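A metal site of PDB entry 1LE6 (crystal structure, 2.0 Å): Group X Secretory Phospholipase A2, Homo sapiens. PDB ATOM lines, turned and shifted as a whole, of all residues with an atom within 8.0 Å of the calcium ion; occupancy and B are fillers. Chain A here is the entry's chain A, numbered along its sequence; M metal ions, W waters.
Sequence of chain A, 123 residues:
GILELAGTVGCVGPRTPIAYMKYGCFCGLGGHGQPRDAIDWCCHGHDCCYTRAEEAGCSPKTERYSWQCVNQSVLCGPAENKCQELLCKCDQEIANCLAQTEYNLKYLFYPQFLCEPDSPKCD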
ATOM      1  N   TYR A  20     -30.689  32.825  10.980  1.00  0.00           N
ATOM      2  CA  TYR A  20     -29.629  32.240  11.796  1.00  0.00           C
ATOM      3  C   TYR A  20     -28.504  31.589  10.990  1.00  0.00           C
ATOM      4  O   TYR A  20     -27.717  30.824  11.547  1.00  0.00           O
ATOM      5  CB  TYR A  20     -30.205  31.200  12.765  1.00  0.00           C
ATOM      6  CG  TYR A  20     -31.472  31.605  13.478  1.00  0.00           C
ATOM      7  CD1 TYR A  20     -32.712  31.176  13.012  1.00  0.00           C
ATOM      8  CD2 TYR A  20     -31.434  32.399  14.619  1.00  0.00           C
ATOM      9  CE1 TYR A  20     -33.893  31.521  13.679  1.00  0.00           C
ATOM     10  CE2 TYR A  20     -32.595  32.751  15.296  1.00  0.00           C
ATOM     11  CZ  TYR A  20     -33.815  32.308  14.829  1.00  0.00           C
ATOM     12  OH  TYR A  20     -34.965  32.646  15.505  1.00  0.00           O
ATOM     13  N   MET A  21     -28.421  31.887   9.698  1.00  0.00           N
ATOM     14  CA  MET A  21     -27.387  31.316   8.847  1.00  0.00           C
ATOM     15  C   MET A  21     -25.991  31.804   9.210  1.00  0.00           C
ATOM     16  O   MET A  21     -25.007  31.071   9.120  1.00  0.00           O
ATOM     17  CB  MET A  21     -27.671  31.603   7.372  1.00  0.00           C
ATOM     18  CG  MET A  21     -28.336  30.455   6.647  1.00  0.00           C
ATOM     19  SD  MET A  21     -28.684  30.817   4.905  1.00  0.00           S
ATOM     20  CE  MET A  21     -27.066  31.294   4.316  1.00  0.00           C
ATOM     21  N   TYR A  23     -24.994  34.221  12.349  1.00  0.00           N
ATOM     22  CA  TYR A  23     -25.349  35.089  13.467  1.00  0.00           C
ATOM     23  C   TYR A  23     -24.469  34.744  14.660  1.00  0.00           C
ATOM     24  O   TYR A  23     -24.279  33.582  14.986  1.00  0.00           O
ATOM     25  CB  TYR A  23     -26.829  34.868  13.800  1.00  0.00           C
ATOM     26  CG  TYR A  23     -27.394  35.710  14.914  1.00  0.00           C
ATOM     27  CD1 TYR A  23     -27.109  35.419  16.253  1.00  0.00           C
ATOM     28  CD2 TYR A  23     -28.256  36.775  14.650  1.00  0.00           C
ATOM     29  CE1 TYR A  23     -27.673  36.156  17.295  1.00  0.00           C
ATOM     30  CE2 TYR A  23     -28.820  37.522  15.672  1.00  0.00           C
ATOM     31  CZ  TYR A  23     -28.533  37.205  16.993  1.00  0.00           C
ATOM     32  OH  TYR A  23     -29.095  37.946  18.007  1.00  0.00           O
ATOM     33  N   CYS A  25     -21.352  34.051  17.162  1.00  0.00           N
ATOM     34  CA  CYS A  25     -20.168  33.215  17.021  1.00  0.00           C
ATOM     35  C   CYS A  25     -20.458  31.739  16.713  1.00  0.00           C
ATOM     36  O   CYS A  25     -19.548  31.019  16.277  1.00  0.00           O
ATOM     37  CB  CYS A  25     -19.303  33.302  18.287  1.00  0.00           C
ATOM     38  SG  CYS A  25     -18.501  34.919  18.506  1.00  0.00           S
ATOM     39  N   PHE A  26     -21.696  31.302  16.898  1.00  0.00           N
ATOM     40  CA  PHE A  26     -22.024  29.887  16.653  1.00  0.00           C
ATOM     41  C   PHE A  26     -23.084  29.552  15.604  1.00  0.00           C
ATOM     42  O   PHE A  26     -23.095  28.432  15.106  1.00  0.00           O
ATOM     43  CB  PHE A  26     -22.383  29.204  17.980  1.00  0.00           C
ATOM     44  CG  PHE A  26     -21.262  29.193  18.971  1.00  0.00           C
ATOM     45  CD1 PHE A  26     -21.012  30.317  19.757  1.00  0.00           C
ATOM     46  CD2 PHE A  26     -20.447  28.086  19.097  1.00  0.00           C
ATOM     47  CE1 PHE A  26     -19.955  30.321  20.653  1.00  0.00           C
ATOM     48  CE2 PHE A  26     -19.379  28.077  19.992  1.00  0.00           C
ATOM     49  CZ  PHE A  26     -19.139  29.201  20.777  1.00  0.00           C
ATOM     50  N   CYS A  27     -23.967  30.480  15.291  1.00  0.00           N
ATOM     51  CA  CYS A  27     -24.982  30.192  14.288  1.00  0.00           C
ATOM     52  C   CYS A  27     -24.312  30.276  12.922  1.00  0.00           C
ATOM     53  O   CYS A  27     -23.994  31.359  12.434  1.00  0.00           O
ATOM     54  CB  CYS A  27     -26.130  31.201  14.376  1.00  0.00           C
ATOM     55  SG  CYS A  27     -26.928  31.260  16.010  1.00  0.00           S
ATOM     56  N   GLY A  28     -24.112  29.126  12.306  1.00  0.00           N
ATOM     57  CA  GLY A  28     -23.440  29.078  11.015  1.00  0.00           C
ATOM     58  C   GLY A  28     -22.335  28.042  11.107  1.00  0.00           C
ATOM     59  O   GLY A  28     -22.137  27.469  12.172  1.00  0.00           O
ATOM     60  N   LEU A  29     -21.620  27.814  10.009  1.00  0.00           N
ATOM     61  CA  LEU A  29     -20.558  26.820   9.988  1.00  0.00           C
ATOM     62  C   LEU A  29     -19.555  26.930  11.138  1.00  0.00           C
ATOM     63  O   LEU A  29     -18.969  27.990  11.366  1.00  0.00           O
ATOM     64  CB  LEU A  29     -19.808  26.875   8.652  1.00  0.00           C
ATOM     65  CG  LEU A  29     -20.662  26.496   7.433  1.00  0.00           C
ATOM     66  CD1 LEU A  29     -19.761  26.352   6.216  1.00  0.00           C
ATOM     67  CD2 LEU A  29     -21.394  25.184   7.697  1.00  0.00           C
ATOM     68  N   GLY A  30     -19.356  25.833  11.846  1.00  0.00           N
ATOM     69  CA  GLY A  30     -18.436  25.821  12.966  1.00  0.00           C
ATOM     70  C   GLY A  30     -18.863  26.805  14.037  1.00  0.00           C
ATOM     71  O   GLY A  30     -20.054  27.055  14.233  1.00  0.00           O
ATOM     72  N   GLY A  31     -17.888  27.383  14.727  1.00  0.00           N
ATOM     73  CA  GLY A  31     -18.191  28.342  15.767  1.00  0.00           C
ATOM     74  C   GLY A  31     -17.341  28.148  16.994  1.00  0.00           C
ATOM     75  O   GLY A  31     -17.080  27.027  17.423  1.00  0.00           O
ATOM     76  N   HIS A  32     -16.904  29.267  17.578  1.00  0.00           N
ATOM     77  CA  HIS A  32     -16.068  29.234  18.768  1.00  0.00           C
ATOM     78  C   HIS A  32     -16.155  30.560  19.502  1.00  0.00           C
ATOM     79  O   HIS A  32     -16.631  31.558  18.940  1.00  0.00           O
ATOM     80  CB  HIS A  32     -14.602  28.967  18.389  1.00  0.00           C
ATOM     81  CG  HIS A  32     -14.038  29.993  17.466  1.00  0.00           C
ATOM     82  ND1 HIS A  32     -14.090  29.866  16.093  1.00  0.00           N
ATOM     83  CD2 HIS A  32     -13.439  31.188  17.707  1.00  0.00           C
ATOM     84  CE1 HIS A  32     -13.555  30.936  15.525  1.00  0.00           C
ATOM     85  NE2 HIS A  32     -13.163  31.752  16.487  1.00  0.00           N
ATOM     86  N   ASP A  40     -27.323  32.859  20.151  1.00  0.00           N
ATOM     87  CA  ASP A  40     -26.024  32.254  19.935  1.00  0.00           C
ATOM     88  C   ASP A  40     -25.836  31.042  20.855  1.00  0.00           C
ATOM     89  O   ASP A  40     -25.180  30.065  20.473  1.00  0.00           O
ATOM     90  CB  ASP A  40     -24.925  33.291  20.174  1.00  0.00           C
ATOM     91  CG  ASP A  40     -23.695  33.063  19.298  1.00  0.00           C
ATOM     92  OD1 ASP A  40     -23.786  32.273  18.325  1.00  0.00           O
ATOM     93  OD2 ASP A  40     -22.640  33.670  19.582  1.00  0.00           O
ATOM     94  N   CYS A  43     -27.489  28.044  19.323  1.00  0.00           N
ATOM     95  CA  CYS A  43     -26.651  27.482  18.266  1.00  0.00           C
ATOM     96  C   CYS A  43     -25.464  26.715  18.843  1.00  0.00           C
ATOM     97  O   CYS A  43     -25.023  25.732  18.253  1.00  0.00           O
ATOM     98  CB  CYS A  43     -26.159  28.587  17.314  1.00  0.00           C
ATOM     99  SG  CYS A  43     -27.508  29.345  16.359  1.00  0.00           S
ATOM    100  N   HIS A  44     -24.958  27.163  19.984  1.00  0.00           N
ATOM    101  CA  HIS A  44     -23.839  26.464  20.616  1.00  0.00           C
ATOM    102  C   HIS A  44     -24.308  25.073  21.044  1.00  0.00           C
ATOM    103  O   HIS A  44     -23.641  24.072  20.796  1.00  0.00           O
ATOM    104  CB  HIS A  44     -23.313  27.240  21.824  1.00  0.00           C
ATOM    105  CG  HIS A  44     -22.346  26.461  22.664  1.00  0.00           C
ATOM    106  ND1 HIS A  44     -22.757  25.560  23.621  1.00  0.00           N
ATOM    107  CD2 HIS A  44     -20.988  26.417  22.658  1.00  0.00           C
ATOM    108  CE1 HIS A  44     -21.697  24.983  24.166  1.00  0.00           C
ATOM    109  NE2 HIS A  44     -20.614  25.492  23.595  1.00  0.00           N
ATOM    110  N   HIS A  46     -26.713  23.478  19.824  1.00  0.00           N
ATOM    111  CA  HIS A  46     -27.029  22.735  18.613  1.00  0.00           C
ATOM    112  C   HIS A  46     -25.732  22.208  17.972  1.00  0.00           C
ATOM    113  O   HIS A  46     -25.701  21.093  17.449  1.00  0.00           O
ATOM    114  CB  HIS A  46     -27.791  23.644  17.634  1.00  0.00           C
ATOM    115  CG  HIS A  46     -28.351  22.912  16.451  1.00  0.00           C
ATOM    116  ND1 HIS A  46     -27.840  23.054  15.174  1.00  0.00           N
ATOM    117  CD2 HIS A  46     -29.408  22.066  16.348  1.00  0.00           C
ATOM    118  CE1 HIS A  46     -28.556  22.325  14.339  1.00  0.00           C
ATOM    119  NE2 HIS A  46     -29.503  21.715  15.027  1.00  0.00           N
ATOM    120  N   ASP A  47     -24.677  23.013  18.004  1.00  0.00           N
ATOM    121  CA  ASP A  47     -23.391  22.572  17.460  1.00  0.00           C
ATOM    122  C   ASP A  47     -22.933  21.355  18.262  1.00  0.00           C
ATOM    123  O   ASP A  47     -22.415  20.387  17.707  1.00  0.00           O
ATOM    124  CB  ASP A  47     -22.346  23.690  17.556  1.00  0.00           C
ATOM    125  CG  ASP A  47     -22.516  24.751  16.488  1.00  0.00           C
ATOM    126  OD1 ASP A  47     -21.648  25.639  16.412  1.00  0.00           O
ATOM    127  OD2 ASP A  47     -23.500  24.697  15.726  1.00  0.00           O
ATOM    128  N   CYS A  48     -23.114  21.413  19.574  1.00  0.00           N
ATOM    129  CA  CYS A  48     -22.737  20.312  20.443  1.00  0.00           C
ATOM    130  C   CYS A  48     -23.515  19.043  20.087  1.00  0.00           C
ATOM    131  O   CYS A  48     -22.956  17.943  20.004  1.00  0.00           O
ATOM    132  CB  CYS A  48     -23.004  20.681  21.899  1.00  0.00           C
ATOM    133  SG  CYS A  48     -21.860  21.900  22.624  1.00  0.00           S
ATOM    134  N   TYR A  50     -25.014  18.293  17.249  1.00  0.00           N
ATOM    135  CA  TYR A  50     -24.602  17.805  15.937  1.00  0.00           C
ATOM    136  C   TYR A  50     -23.277  17.064  16.005  1.00  0.00           C
ATOM    137  O   TYR A  50     -23.079  16.059  15.316  1.00  0.00           O
ATOM    138  CB  TYR A  50     -24.511  18.971  14.944  1.00  0.00           C
ATOM    139  CG  TYR A  50     -25.764  19.181  14.128  1.00  0.00           C
ATOM    140  CD1 TYR A  50     -26.995  18.650  14.536  1.00  0.00           C
ATOM    141  CD2 TYR A  50     -25.728  19.900  12.927  1.00  0.00           C
ATOM    142  CE1 TYR A  50     -28.150  18.816  13.764  1.00  0.00           C
ATOM    143  CE2 TYR A  50     -26.882  20.074  12.150  1.00  0.00           C
ATOM    144  CZ  TYR A  50     -28.084  19.535  12.580  1.00  0.00           C
ATOM    145  OH  TYR A  50     -29.208  19.696  11.802  1.00  0.00           O
ATOM    146  N   GLN A 112     -16.723  36.463  12.323  1.00  0.00           N
ATOM    147  CA  GLN A 112     -16.186  35.336  13.078  1.00  0.00           C
ATOM    148  C   GLN A 112     -14.806  35.568  13.684  1.00  0.00           C
ATOM    149  O   GLN A 112     -14.487  34.990  14.729  1.00  0.00           O
ATOM    150  CB  GLN A 112     -16.152  34.082  12.208  1.00  0.00           C
ATOM    151  CG  GLN A 112     -15.668  32.847  12.938  1.00  0.00           C
ATOM    152  CD  GLN A 112     -16.652  31.696  12.849  1.00  0.00           C
ATOM    153  OE1 GLN A 112     -17.811  31.807  13.242  1.00  0.00           O
ATOM    154  NE2 GLN A 112     -16.189  30.563  12.325  1.00  0.00           N
HETATM  155 CA    CA M   1     -22.334  26.442  14.221  1.00  0.00          CA
HETATM  156  O   HOH W   1     -24.664  26.288  13.260  1.00  0.00           O
HETATM  157  O   HOH W   2     -21.805  24.404  13.120  1.00  0.00           O
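The backbone NH of Phe 26 lies within hydrogen-bond range of the side-chain carboxylate of Asp 40.
SG of Cys 27 forms a disulfide with SG of Cys 43, at 2.0 Å.
Within 4 Å of the calcium ion: Phe 26, Gly 28, Gly 30 and Asp 47.
The calcium ion is bound by O of Gly 28 (2.3 Å), O of Phe 26 (2.3 Å), O of Gly 30 (2.4 Å), water W2 (2.4 Å), OD1 of Asp 47 (2.4 Å), water W1 (2.5 Å) and OD2 of Asp 47 (2.6 Å).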
